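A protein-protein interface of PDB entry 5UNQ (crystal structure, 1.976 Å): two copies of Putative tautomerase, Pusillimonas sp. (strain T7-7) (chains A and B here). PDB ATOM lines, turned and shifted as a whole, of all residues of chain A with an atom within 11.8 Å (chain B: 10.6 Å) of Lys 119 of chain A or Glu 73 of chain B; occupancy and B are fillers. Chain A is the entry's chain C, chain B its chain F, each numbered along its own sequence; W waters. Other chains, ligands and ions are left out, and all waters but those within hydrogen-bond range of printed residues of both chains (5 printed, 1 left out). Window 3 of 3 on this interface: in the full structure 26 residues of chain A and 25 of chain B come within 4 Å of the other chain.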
ATOM      1  N   PHE A  67      -4.720 -24.580  18.600  1.00  0.00           N
ATOM      2  CA  PHE A  67      -3.378 -24.483  18.038  1.00  0.00           C
ATOM      3  C   PHE A  67      -2.971 -25.761  17.309  1.00  0.00           C
ATOM      4  O   PHE A  67      -3.633 -26.792  17.427  1.00  0.00           O
ATOM      5  CB  PHE A  67      -2.376 -24.137  19.144  1.00  0.00           C
ATOM      6  CG  PHE A  67      -1.934 -25.316  19.970  1.00  0.00           C
ATOM      7  CD1 PHE A  67      -0.590 -25.651  20.063  1.00  0.00           C
ATOM      8  CD2 PHE A  67      -2.859 -26.092  20.644  1.00  0.00           C
ATOM      9  CE1 PHE A  67      -0.179 -26.737  20.810  1.00  0.00           C
ATOM     10  CE2 PHE A  67      -2.453 -27.172  21.405  1.00  0.00           C
ATOM     11  CZ  PHE A  67      -1.107 -27.491  21.491  1.00  0.00           C
ATOM     12  N   ILE A  68      -1.893 -25.672  16.538  1.00  0.00           N
ATOM     13  CA  ILE A  68      -1.431 -26.775  15.701  1.00  0.00           C
ATOM     14  C   ILE A  68      -0.731 -27.854  16.527  1.00  0.00           C
ATOM     15  O   ILE A  68      -0.048 -27.550  17.507  1.00  0.00           O
ATOM     16  CB  ILE A  68      -0.475 -26.263  14.592  1.00  0.00           C
ATOM     17  CG1 ILE A  68      -1.189 -25.247  13.699  1.00  0.00           C
ATOM     18  CG2 ILE A  68       0.068 -27.408  13.746  1.00  0.00           C
ATOM     19  CD1 ILE A  68      -0.354 -24.771  12.529  1.00  0.00           C
ATOM     20  N   GLU A  69      -0.918 -29.113  16.132  1.00  0.00           N
ATOM     21  CA  GLU A  69      -0.200 -30.240  16.721  1.00  0.00           C
ATOM     22  C   GLU A  69       1.312 -30.040  16.719  1.00  0.00           C
ATOM     23  O   GLU A  69       1.840 -29.216  15.974  1.00  0.00           O
ATOM     24  CB  GLU A  69      -0.517 -31.531  15.968  1.00  0.00           C
ATOM     25  CG  GLU A  69      -1.954 -31.989  16.041  1.00  0.00           C
ATOM     26  CD  GLU A  69      -2.181 -33.254  15.238  1.00  0.00           C
ATOM     27  OE1 GLU A  69      -1.399 -33.503  14.297  1.00  0.00           O
ATOM     28  OE2 GLU A  69      -3.131 -34.000  15.551  1.00  0.00           O
ATOM     29  N   PHE A 105      -4.890 -29.056  16.342  1.00  0.00           N
ATOM     30  CA  PHE A 105      -5.341 -29.047  14.959  1.00  0.00           C
ATOM     31  C   PHE A 105      -4.245 -29.591  14.055  1.00  0.00           C
ATOM     32  O   PHE A 105      -3.096 -29.163  14.147  1.00  0.00           O
ATOM     33  CB  PHE A 105      -5.726 -27.634  14.514  1.00  0.00           C
ATOM     34  CG  PHE A 105      -7.058 -27.170  15.032  1.00  0.00           C
ATOM     35  CD1 PHE A 105      -7.214 -26.801  16.357  1.00  0.00           C
ATOM     36  CD2 PHE A 105      -8.152 -27.085  14.186  1.00  0.00           C
ATOM     37  CE1 PHE A 105      -8.439 -26.366  16.831  1.00  0.00           C
ATOM     38  CE2 PHE A 105      -9.378 -26.653  14.653  1.00  0.00           C
ATOM     39  CZ  PHE A 105      -9.522 -26.291  15.977  1.00  0.00           C
ATOM     40  N   PRO A 106      -4.589 -30.548  13.185  1.00  0.00           N
ATOM     41  CA  PRO A 106      -3.611 -30.958  12.174  1.00  0.00           C
ATOM     42  C   PRO A 106      -3.332 -29.806  11.217  1.00  0.00           C
ATOM     43  O   PRO A 106      -4.199 -28.950  11.036  1.00  0.00           O
ATOM     44  CB  PRO A 106      -4.296 -32.129  11.465  1.00  0.00           C
ATOM     45  CG  PRO A 106      -5.752 -31.943  11.733  1.00  0.00           C
ATOM     46  CD  PRO A 106      -5.842 -31.315  13.092  1.00  0.00           C
ATOM     47  N   LYS A 107      -2.143 -29.778  10.625  1.00  0.00           N
ATOM     48  CA  LYS A 107      -1.763 -28.704   9.711  1.00  0.00           C
ATOM     49  C   LYS A 107      -2.713 -28.609   8.520  1.00  0.00           C
ATOM     50  O   LYS A 107      -2.869 -27.544   7.924  1.00  0.00           O
ATOM     51  CB  LYS A 107      -0.328 -28.904   9.221  1.00  0.00           C
ATOM     52  CG  LYS A 107       0.725 -28.648  10.282  1.00  0.00           C
ATOM     53  CD  LYS A 107       2.108 -29.057   9.804  1.00  0.00           C
ATOM     54  CE  LYS A 107       3.159 -28.770  10.861  1.00  0.00           C
ATOM     55  NZ  LYS A 107       4.493 -29.312  10.478  1.00  0.00           N
ATOM     56  N   ALA A 108      -3.346 -29.726   8.181  1.00  0.00           N
ATOM     57  CA  ALA A 108      -4.291 -29.768   7.074  1.00  0.00           C
ATOM     58  C   ALA A 108      -5.564 -28.982   7.383  1.00  0.00           C
ATOM     59  O   ALA A 108      -6.233 -28.493   6.472  1.00  0.00           O
ATOM     60  CB  ALA A 108      -4.635 -31.210   6.731  1.00  0.00           C
ATOM     61  N   ASN A 109      -5.893 -28.858   8.666  1.00  0.00           N
ATOM     62  CA  ASN A 109      -7.145 -28.224   9.074  1.00  0.00           C
ATOM     63  C   ASN A 109      -6.991 -26.783   9.554  1.00  0.00           C
ATOM     64  O   ASN A 109      -7.981 -26.064   9.696  1.00  0.00           O
ATOM     65  CB  ASN A 109      -7.817 -29.047  10.175  1.00  0.00           C
ATOM     66  CG  ASN A 109      -8.286 -30.402   9.685  1.00  0.00           C
ATOM     67  OD1 ASN A 109      -8.247 -30.688   8.491  1.00  0.00           O
ATOM     68  ND2 ASN A 109      -8.746 -31.239  10.609  1.00  0.00           N
ATOM     69  N   MET A 110      -5.757 -26.361   9.808  1.00  0.00           N
ATOM     70  CA  MET A 110      -5.514 -25.019  10.326  1.00  0.00           C
ATOM     71  C   MET A 110      -5.206 -24.029   9.209  1.00  0.00           C
ATOM     72  O   MET A 110      -4.098 -24.003   8.675  1.00  0.00           O
ATOM     73  CB  MET A 110      -4.370 -25.035  11.341  1.00  0.00           C
ATOM     74  CG  MET A 110      -4.054 -23.670  11.939  1.00  0.00           C
ATOM     75  SD  MET A 110      -5.405 -23.008  12.933  1.00  0.00           S
ATOM     76  CE  MET A 110      -5.298 -24.037  14.393  1.00  0.00           C
ATOM     77  N   GLY A 111      -6.195 -23.212   8.862  1.00  0.00           N
ATOM     78  CA  GLY A 111      -6.011 -22.192   7.848  1.00  0.00           C
ATOM     79  C   GLY A 111      -5.108 -21.081   8.346  1.00  0.00           C
ATOM     80  O   GLY A 111      -5.084 -20.767   9.538  1.00  0.00           O
ATOM     81  N   MET A 112      -4.355 -20.490   7.426  1.00  0.00           N
ATOM     82  CA  MET A 112      -3.439 -19.411   7.764  1.00  0.00           C
ATOM     83  C   MET A 112      -3.794 -18.162   6.969  1.00  0.00           C
ATOM     84  O   MET A 112      -4.910 -18.037   6.458  1.00  0.00           O
ATOM     85  CB  MET A 112      -1.995 -19.829   7.481  1.00  0.00           C
ATOM     86  CG  MET A 112      -1.608 -21.190   8.041  1.00  0.00           C
ATOM     87  SD  MET A 112      -1.434 -21.197   9.835  1.00  0.00           S
ATOM     88  CE  MET A 112       0.064 -20.229  10.018  1.00  0.00           C
ATOM     89  N   ALA A 113      -2.841 -17.244   6.856  1.00  0.00           N
ATOM     90  CA  ALA A 113      -3.040 -16.043   6.054  1.00  0.00           C
ATOM     91  C   ALA A 113      -3.123 -16.398   4.573  1.00  0.00           C
ATOM     92  O   ALA A 113      -2.357 -17.227   4.082  1.00  0.00           O
ATOM     93  CB  ALA A 113      -1.920 -15.043   6.301  1.00  0.00           C
ATOM     94  N   GLY A 114      -4.061 -15.774   3.867  1.00  0.00           N
ATOM     95  CA  GLY A 114      -4.209 -15.994   2.440  1.00  0.00           C
ATOM     96  C   GLY A 114      -5.121 -17.154   2.090  1.00  0.00           C
ATOM     97  O   GLY A 114      -5.156 -17.598   0.942  1.00  0.00           O
ATOM     98  N   GLY A 115      -5.858 -17.648   3.079  1.00  0.00           N
ATOM     99  CA  GLY A 115      -6.812 -18.721   2.860  1.00  0.00           C
ATOM    100  C   GLY A 115      -6.188 -20.050   2.474  1.00  0.00           C
ATOM    101  O   GLY A 115      -6.764 -20.811   1.696  1.00  0.00           O
ATOM    102  N   ILE A 116      -5.006 -20.328   3.014  1.00  0.00           N
ATOM    103  CA  ILE A 116      -4.338 -21.603   2.769  1.00  0.00           C
ATOM    104  C   ILE A 116      -3.939 -22.267   4.085  1.00  0.00           C
ATOM    105  O   ILE A 116      -3.572 -21.591   5.047  1.00  0.00           O
ATOM    106  CB  ILE A 116      -3.087 -21.432   1.880  1.00  0.00           C
ATOM    107  CG1 ILE A 116      -2.107 -20.443   2.512  1.00  0.00           C
ATOM    108  CG2 ILE A 116      -3.483 -20.967   0.487  1.00  0.00           C
ATOM    109  CD1 ILE A 116      -0.821 -20.275   1.734  1.00  0.00           C
ATOM    110  N   SER A 117      -4.020 -23.593   4.122  1.00  0.00           N
ATOM    111  CA  SER A 117      -3.721 -24.341   5.338  1.00  0.00           C
ATOM    112  C   SER A 117      -2.225 -24.350   5.637  1.00  0.00           C
ATOM    113  O   SER A 117      -1.406 -24.030   4.774  1.00  0.00           O
ATOM    114  CB  SER A 117      -4.236 -25.778   5.229  1.00  0.00           C
ATOM    115  OG  SER A 117      -3.485 -26.520   4.282  1.00  0.00           O
ATOM    116  N   ALA A 118      -1.880 -24.732   6.862  1.00  0.00           N
ATOM    117  CA  ALA A 118      -0.490 -24.775   7.296  1.00  0.00           C
ATOM    118  C   ALA A 118       0.297 -25.835   6.533  1.00  0.00           C
ATOM    119  O   ALA A 118       1.483 -25.661   6.259  1.00  0.00           O
ATOM    120  CB  ALA A 118      -0.410 -25.031   8.794  1.00  0.00           C
ATOM    121  N   LYS A 119      -0.371 -26.932   6.189  1.00  0.00           N
ATOM    122  CA  LYS A 119       0.271 -28.011   5.449  1.00  0.00           C
ATOM    123  C   LYS A 119       0.633 -27.575   4.034  1.00  0.00           C
ATOM    124  O   LYS A 119       1.758 -27.782   3.581  1.00  0.00           O
ATOM    125  CB  LYS A 119      -0.632 -29.246   5.402  1.00  0.00           C
ATOM    126  CG  LYS A 119      -0.092 -30.359   4.520  1.00  0.00           C
ATOM    127  CD  LYS A 119      -0.986 -31.587   4.553  1.00  0.00           C
ATOM    128  CE  LYS A 119      -0.341 -32.750   3.816  1.00  0.00           C
ATOM    129  NZ  LYS A 119      -0.703 -34.064   4.414  1.00  0.00           N
ATOM    130  N   ALA A 120      -0.327 -26.970   3.340  1.00  0.00           N
ATOM    131  CA  ALA A 120      -0.103 -26.483   1.983  1.00  0.00           C
ATOM    132  C   ALA A 120       0.925 -25.354   1.974  1.00  0.00           C
ATOM    133  O   ALA A 120       1.635 -25.154   0.989  1.00  0.00           O
ATOM    134  CB  ALA A 120      -1.412 -26.016   1.363  1.00  0.00           C
ATOM    135  N   MET A 121       0.996 -24.623   3.081  1.00  0.00           N
ATOM    136  CA  MET A 121       1.957 -23.536   3.228  1.00  0.00           C
ATOM    137  C   MET A 121       3.389 -24.062   3.282  1.00  0.00           C
ATOM    138  O   MET A 121       4.328 -23.380   2.870  1.00  0.00           O
ATOM    139  CB  MET A 121       1.638 -22.718   4.480  1.00  0.00           C
ATOM    140  CG  MET A 121       2.574 -21.548   4.721  1.00  0.00           C
ATOM    141  SD  MET A 121       2.020 -20.499   6.074  1.00  0.00           S
ATOM    142  CE  MET A 121       0.722 -19.586   5.248  1.00  0.00           C
ATOM    143  N   GLY A 122       3.548 -25.281   3.785  1.00  0.00           N
ATOM    144  CA  GLY A 122       4.850 -25.918   3.853  1.00  0.00           C
ATOM    145  C   GLY A 122       5.805 -25.212   4.794  1.00  0.00           C
ATOM    146  O   GLY A 122       6.216 -25.772   5.810  1.00  0.00           O
ATOM    147  N   SER B  30     -18.247 -25.816  -1.721  1.00  0.00           N
ATOM    148  CA  SER B  30     -16.933 -26.375  -1.410  1.00  0.00           C
ATOM    149  C   SER B  30     -16.960 -27.891  -1.258  1.00  0.00           C
ATOM    150  O   SER B  30     -16.270 -28.606  -1.984  1.00  0.00           O
ATOM    151  CB  SER B  30     -16.370 -25.748  -0.133  1.00  0.00           C
ATOM    152  OG  SER B  30     -16.189 -24.352  -0.285  1.00  0.00           O
ATOM    153  N   ILE B  31     -17.752 -28.377  -0.309  1.00  0.00           N
ATOM    154  CA  ILE B  31     -17.752 -29.797   0.024  1.00  0.00           C
ATOM    155  C   ILE B  31     -19.059 -30.491  -0.353  1.00  0.00           C
ATOM    156  O   ILE B  31     -19.308 -31.624   0.060  1.00  0.00           O
ATOM    157  CB  ILE B  31     -17.484 -30.014   1.525  1.00  0.00           C
ATOM    158  CG1 ILE B  31     -18.602 -29.392   2.365  1.00  0.00           C
ATOM    159  CG2 ILE B  31     -16.135 -29.427   1.913  1.00  0.00           C
ATOM    160  CD1 ILE B  31     -18.441 -29.618   3.853  1.00  0.00           C
ATOM    161  N   PHE B  67     -17.422 -30.212  11.698  1.00  0.00           N
ATOM    162  CA  PHE B  67     -17.996 -31.145  10.734  1.00  0.00           C
ATOM    163  C   PHE B  67     -17.562 -32.586  10.976  1.00  0.00           C
ATOM    164  O   PHE B  67     -16.591 -32.845  11.685  1.00  0.00           O
ATOM    165  CB  PHE B  67     -17.633 -30.718   9.308  1.00  0.00           C
ATOM    166  CG  PHE B  67     -16.191 -30.948   8.943  1.00  0.00           C
ATOM    167  CD1 PHE B  67     -15.835 -32.005   8.127  1.00  0.00           C
ATOM    168  CD2 PHE B  67     -15.194 -30.105   9.407  1.00  0.00           C
ATOM    169  CE1 PHE B  67     -14.514 -32.219   7.777  1.00  0.00           C
ATOM    170  CE2 PHE B  67     -13.870 -30.317   9.060  1.00  0.00           C
ATOM    171  CZ  PHE B  67     -13.532 -31.378   8.250  1.00  0.00           C
ATOM    172  N   GLU B  69     -15.791 -35.962  10.414  1.00  0.00           N
ATOM    173  CA  GLU B  69     -14.514 -36.339   9.814  1.00  0.00           C
ATOM    174  C   GLU B  69     -14.708 -37.152   8.537  1.00  0.00           C
ATOM    175  O   GLU B  69     -15.748 -37.784   8.343  1.00  0.00           O
ATOM    176  CB  GLU B  69     -13.670 -37.135  10.811  1.00  0.00           C
ATOM    177  CG  GLU B  69     -14.257 -38.490  11.175  1.00  0.00           C
ATOM    178  CD  GLU B  69     -13.324 -39.318  12.036  1.00  0.00           C
ATOM    179  OE1 GLU B  69     -13.705 -40.445  12.415  1.00  0.00           O
ATOM    180  OE2 GLU B  69     -12.209 -38.841  12.335  1.00  0.00           O
ATOM    181  N   GLY B  70     -13.708 -37.125   7.663  1.00  0.00           N
ATOM    182  CA  GLY B  70     -13.744 -37.926   6.452  1.00  0.00           C
ATOM    183  C   GLY B  70     -13.574 -37.150   5.160  1.00  0.00           C
ATOM    184  O   GLY B  70     -13.402 -37.748   4.099  1.00  0.00           O
ATOM    185  N   ARG B  71     -13.626 -35.824   5.239  1.00  0.00           N
ATOM    186  CA  ARG B  71     -13.444 -34.990   4.054  1.00  0.00           C
ATOM    187  C   ARG B  71     -12.033 -35.127   3.487  1.00  0.00           C
ATOM    188  O   ARG B  71     -11.065 -35.271   4.232  1.00  0.00           O
ATOM    189  CB  ARG B  71     -13.740 -33.523   4.372  1.00  0.00           C
ATOM    190  CG  ARG B  71     -15.159 -33.082   4.045  1.00  0.00           C
ATOM    191  CD  ARG B  71     -16.160 -33.595   5.064  1.00  0.00           C
ATOM    192  NE  ARG B  71     -17.529 -33.232   4.713  1.00  0.00           N
ATOM    193  CZ  ARG B  71     -18.555 -33.275   5.557  1.00  0.00           C
ATOM    194  NH1 ARG B  71     -19.768 -32.926   5.150  1.00  0.00           N
ATOM    195  NH2 ARG B  71     -18.366 -33.658   6.813  1.00  0.00           N
ATOM    196  N   THR B  72     -11.924 -35.086   2.163  1.00  0.00           N
ATOM    197  CA  THR B  72     -10.629 -35.203   1.500  1.00  0.00           C
ATOM    198  C   THR B  72      -9.849 -33.897   1.601  1.00  0.00           C
ATOM    199  O   THR B  72     -10.419 -32.849   1.908  1.00  0.00           O
ATOM    200  CB  THR B  72     -10.782 -35.583   0.018  1.00  0.00           C
ATOM    201  OG1 THR B  72     -11.279 -34.457  -0.716  1.00  0.00           O
ATOM    202  CG2 THR B  72     -11.742 -36.753  -0.134  1.00  0.00           C
ATOM    203  N   GLU B  73      -8.547 -33.965   1.338  1.00  0.00           N
ATOM    204  CA  GLU B  73      -7.687 -32.787   1.401  1.00  0.00           C
ATOM    205  C   GLU B  73      -8.144 -31.697   0.438  1.00  0.00           C
ATOM    206  O   GLU B  73      -8.099 -30.511   0.766  1.00  0.00           O
ATOM    207  CB  GLU B  73      -6.233 -33.158   1.102  1.00  0.00           C
ATOM    208  CG  GLU B  73      -5.526 -33.888   2.230  1.00  0.00           C
ATOM    209  CD  GLU B  73      -4.016 -33.813   2.109  1.00  0.00           C
ATOM    210  OE1 GLU B  73      -3.525 -33.115   1.198  1.00  0.00           O
ATOM    211  OE2 GLU B  73      -3.319 -34.450   2.928  1.00  0.00           O
ATOM    212  N   GLU B  74      -8.581 -32.105  -0.749  1.00  0.00           N
ATOM    213  CA  GLU B  74      -9.045 -31.156  -1.753  1.00  0.00           C
ATOM    214  C   GLU B  74     -10.290 -30.419  -1.267  1.00  0.00           C
ATOM    215  O   GLU B  74     -10.455 -29.226  -1.521  1.00  0.00           O
ATOM    216  CB  GLU B  74      -9.327 -31.866  -3.080  1.00  0.00           C
ATOM    217  CG  GLU B  74      -9.700 -30.924  -4.211  1.00  0.00           C
ATOM    218  CD  GLU B  74      -9.606 -31.574  -5.578  1.00  0.00           C
ATOM    219  OE1 GLU B  74      -9.846 -32.795  -5.678  1.00  0.00           O
ATOM    220  OE2 GLU B  74      -9.290 -30.860  -6.553  1.00  0.00           O
ATOM    221  N   GLN B  75     -11.156 -31.135  -0.557  1.00  0.00           N
ATOM    222  CA  GLN B  75     -12.369 -30.543  -0.004  1.00  0.00           C
ATOM    223  C   GLN B  75     -12.047 -29.547   1.107  1.00  0.00           C
ATOM    224  O   GLN B  75     -12.695 -28.508   1.225  1.00  0.00           O
ATOM    225  CB  GLN B  75     -13.302 -31.630   0.530  1.00  0.00           C
ATOM    226  CG  GLN B  75     -13.885 -32.534  -0.539  1.00  0.00           C
ATOM    227  CD  GLN B  75     -14.808 -33.588   0.036  1.00  0.00           C
ATOM    228  OE1 GLN B  75     -14.367 -34.499   0.737  1.00  0.00           O
ATOM    229  NE2 GLN B  75     -16.098 -33.469  -0.257  1.00  0.00           N
ATOM    230  N   ARG B  76     -11.050 -29.875   1.922  1.00  0.00           N
ATOM    231  CA  ARG B  76     -10.643 -29.009   3.022  1.00  0.00           C
ATOM    232  C   ARG B  76     -10.036 -27.711   2.508  1.00  0.00           C
ATOM    233  O   ARG B  76     -10.393 -26.624   2.964  1.00  0.00           O
ATOM    234  CB  ARG B  76      -9.641 -29.723   3.929  1.00  0.00           C
ATOM    235  CG  ARG B  76     -10.150 -31.019   4.524  1.00  0.00           C
ATOM    236  CD  ARG B  76      -9.044 -31.727   5.286  1.00  0.00           C
ATOM    237  NE  ARG B  76      -9.540 -32.893   6.008  1.00  0.00           N
ATOM    238  CZ  ARG B  76     -10.148 -32.835   7.189  1.00  0.00           C
ATOM    239  NH1 ARG B  76     -10.339 -31.664   7.781  1.00  0.00           N
ATOM    240  NH2 ARG B  76     -10.567 -33.946   7.777  1.00  0.00           N
ATOM    241  N   ASN B  77      -9.113 -27.834   1.561  1.00  0.00           N
ATOM    242  CA  ASN B  77      -8.465 -26.671   0.968  1.00  0.00           C
ATOM    243  C   ASN B  77      -9.463 -25.770   0.253  1.00  0.00           C
ATOM    244  O   ASN B  77      -9.332 -24.548   0.274  1.00  0.00           O
ATOM    245  CB  ASN B  77      -7.365 -27.111   0.002  1.00  0.00           C
ATOM    246  CG  ASN B  77      -6.143 -27.657   0.718  1.00  0.00           C
ATOM    247  OD1 ASN B  77      -6.106 -27.719   1.947  1.00  0.00           O
ATOM    248  ND2 ASN B  77      -5.138 -28.062  -0.050  1.00  0.00           N
ATOM    249  N   ALA B  78     -10.463 -26.379  -0.375  1.00  0.00           N
ATOM    250  CA  ALA B  78     -11.504 -25.627  -1.066  1.00  0.00           C
ATOM    251  C   ALA B  78     -12.402 -24.903  -0.069  1.00  0.00           C
ATOM    252  O   ALA B  78     -12.866 -23.793  -0.328  1.00  0.00           O
ATOM    253  CB  ALA B  78     -12.330 -26.548  -1.951  1.00  0.00           C
ATOM    254  N   LEU B  79     -12.641 -25.540   1.074  1.00  0.00           N
ATOM    255  CA  LEU B  79     -13.485 -24.960   2.111  1.00  0.00           C
ATOM    256  C   LEU B  79     -12.796 -23.779   2.787  1.00  0.00           C
ATOM    257  O   LEU B  79     -13.406 -22.731   2.998  1.00  0.00           O
ATOM    258  CB  LEU B  79     -13.859 -26.018   3.150  1.00  0.00           C
ATOM    259  CG  LEU B  79     -14.743 -25.550   4.308  1.00  0.00           C
ATOM    260  CD1 LEU B  79     -16.035 -24.942   3.785  1.00  0.00           C
ATOM    261  CD2 LEU B  79     -15.036 -26.703   5.254  1.00  0.00           C
ATOM    262  N   ILE B  80     -11.523 -23.961   3.124  1.00  0.00           N
ATOM    263  CA  ILE B  80     -10.728 -22.906   3.741  1.00  0.00           C
ATOM    264  C   ILE B  80     -10.618 -21.699   2.813  1.00  0.00           C
ATOM    265  O   ILE B  80     -10.732 -20.554   3.250  1.00  0.00           O
ATOM    266  CB  ILE B  80      -9.312 -23.408   4.104  1.00  0.00           C
ATOM    267  CG1 ILE B  80      -9.392 -24.502   5.172  1.00  0.00           C
ATOM    268  CG2 ILE B  80      -8.435 -22.260   4.589  1.00  0.00           C
ATOM    269  CD1 ILE B  80      -8.063 -25.165   5.474  1.00  0.00           C
ATOM    270  N   ALA B  81     -10.418 -21.968   1.527  1.00  0.00           N
ATOM    271  CA  ALA B  81     -10.251 -20.908   0.536  1.00  0.00           C
ATOM    272  C   ALA B  81     -11.548 -20.141   0.284  1.00  0.00           C
ATOM    273  O   ALA B  81     -11.540 -18.914   0.182  1.00  0.00           O
ATOM    274  CB  ALA B  81      -9.723 -21.489  -0.768  1.00  0.00           C
ATOM    275  N   VAL B 100      -9.477 -19.292   8.995  1.00  0.00           N
ATOM    276  CA  VAL B 100     -10.470 -20.368   8.950  1.00  0.00           C
ATOM    277  C   VAL B 100      -9.913 -21.653   9.566  1.00  0.00           C
ATOM    278  O   VAL B 100      -8.846 -22.117   9.172  1.00  0.00           O
ATOM    279  CB  VAL B 100     -10.929 -20.671   7.503  1.00  0.00           C
ATOM    280  CG1 VAL B 100     -11.926 -21.823   7.492  1.00  0.00           C
ATOM    281  CG2 VAL B 100     -11.536 -19.435   6.854  1.00  0.00           C
ATOM    282  N   LEU B 102     -10.694 -25.824  10.764  1.00  0.00           N
ATOM    283  CA  LEU B 102     -11.550 -26.992  10.577  1.00  0.00           C
ATOM    284  C   LEU B 102     -11.434 -27.966  11.746  1.00  0.00           C
ATOM    285  O   LEU B 102     -10.336 -28.379  12.111  1.00  0.00           O
ATOM    286  CB  LEU B 102     -11.208 -27.712   9.271  1.00  0.00           C
ATOM    287  CG  LEU B 102     -11.274 -26.890   7.984  1.00  0.00           C
ATOM    288  CD1 LEU B 102     -11.063 -27.781   6.769  1.00  0.00           C
ATOM    289  CD2 LEU B 102     -12.592 -26.142   7.889  1.00  0.00           C
ATOM    290  N   ASP B 104     -12.632 -31.674  13.168  1.00  0.00           N
ATOM    291  CA  ASP B 104     -13.182 -32.984  12.820  1.00  0.00           C
ATOM    292  C   ASP B 104     -13.978 -33.623  13.951  1.00  0.00           C
ATOM    293  O   ASP B 104     -13.633 -33.483  15.120  1.00  0.00           O
ATOM    294  CB  ASP B 104     -12.055 -33.934  12.402  1.00  0.00           C
ATOM    295  CG  ASP B 104     -11.516 -33.628  11.018  1.00  0.00           C
ATOM    296  OD1 ASP B 104     -12.327 -33.285  10.131  1.00  0.00           O
ATOM    297  OD2 ASP B 104     -10.284 -33.721  10.820  1.00  0.00           O
HETATM  298  O   HOH W   1      -4.877 -25.021   1.885  1.00  0.00           O
HETATM  299  O   HOH W   2      -4.708 -28.562   3.932  1.00  0.00           O
HETATM  300  O   HOH W   3      -7.082 -19.125   6.737  1.00  0.00           O
HETATM  301  O   HOH W   4      -9.697 -32.125  13.841  1.00  0.00           O
HETATM  302  O   HOH W   5      -6.945 -23.559   0.896  1.00  0.00           O
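The side-chain amino group (NZ) of Lys 119 of chain A lies within salt-bridge range of the side-chain carboxylate (OE2) of Glu 73 of chain B (3.0 Å). NH1 of Arg 76 of chain B lies within hydrogen-bond range of OD1 of Asn 109 of chain A (2.4 Å). N of Gly 111 of chain A sits at hydrogen-bond distance from O of Val 100 of chain B. The backbone NH (N) of Leu 102 of chain B sits at hydrogen-bond distance from the backbone carbonyl oxygen (O) of Asn 109 of chain A (2.9 Å). OD2 of Asp 104 of chain B sits at hydrogen-bond distance from ND2 of Asn 109 of chain A.
The backbone carbonyl oxygen (O) of Arg 71 of chain B lies within hydrogen-bond range of the guanidinium group (NE) of Arg 76 of chain B (3.3 Å). The guanidinium group (NH2) of Arg 76 of chain B lies within salt-bridge range of the side-chain carboxylate (OD1) of Asp 104 of chain B (3.0 Å). O of Phe 105 of chain A sits at hydrogen-bond distance from N of Glu 69 of chain A (2.9 Å). N of Lys 119 of chain A is in hydrogen-bond range of O of Lys 107 of chain A, at 3.1 Å. OG of Ser 117 of chain A is in hydrogen-bond range of N of Ala 120 of chain A.
Phe 105 of chain A touches Leu 102 of chain B. Ala 108 of chain A touches Ile 80 of chain B (O to CD1, 3.9 Å). O of Gly 115 of chain A touches CG2 of Ile 80 of chain B, at 3.6 Å. O of Gly 115 of chain A touches CA of Ala 81 of chain B (3.7 Å). OG of Ser 117 of chain A touches OD1 of Asn 77 of chain B, 3.7 Å away. Ser 117 of chain A touches Ile 80 of chain B.
Of the printed residues of chain B, Phe 105 of chain A touches Leu 102 (3.2 Å). Ala 108 of chain A touches just one residue of chain B: Ile 80 (3.9 Å). Met 112 of chain A touches none of the printed residues of chain B. Ser 117 of chain A touches just these residues of chain B: Asn 77 (3.7 Å) and Ile 80 (3.9 Å). No residue of chain B comes within 4 Å of Ala 118 of chain A. No residue of chain A comes within 4 Å of Thr 72 of chain B. Glu 73 of chain B touches just one residue of chain A: Lys 119. No residue of chain A comes within 4 Å of Gln 75 of chain B. Arg 76 of chain B touches just one residue of chain A: Asn 109. Ala 78 of chain B touches none of the printed residues of chain A. Printed residues of chain A within 4 Å of Ala 81 of chain B: Gly 115 (3.7 Å). Printed residues of chain A within 4 Å of Val 100 of chain B: Gly 111. Printed residues of chain A within 4 Å of Leu 102 of chain B: Phe 105 (3.2 Å) and Asn 109 (2.9 Å).
Of the 19 printed residues of chain B, 8 touch a printed residue of chain A. Printed residues of chain B that touch a printed residue of chain A: Glu 73, Arg 76, Asn 77, Ile 80, Ala 81, Val 100, Leu 102 and Asp 104. Of the 21 printed residues of chain A, 7 touch a printed residue of chain B. Hydrophobic or aromatic side chains of chain A that line the printed part of chain B: Phe 105. Among the printed residues, Asp or Glu carboxylates within 4 Å of a Lys or Arg side-chain nitrogen of the other chain: Lys 119 of chain A with Glu 73 of chain B (3.0 Å).
2 positions are printed for both chains.
Water W2 lies within hydrogen-bond range of the side-chain hydroxyl of Ser 117 of chain A, the side-chain amide oxygen of Asn 77 of chain B and the backbone carbonyl oxygen of Ala 108 of chain A. Water W3 lies within hydrogen-bond range of the backbone carbonyl oxygen (O) of Met 112 of chain A and the backbone NH (N) of Val 100 of chain B. Water W4 bridges the backbone NH of Asp 104 of chain B (3.0 Å) and the side-chain amide nitrogen of Asn 109 of chain A (3.5 Å).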
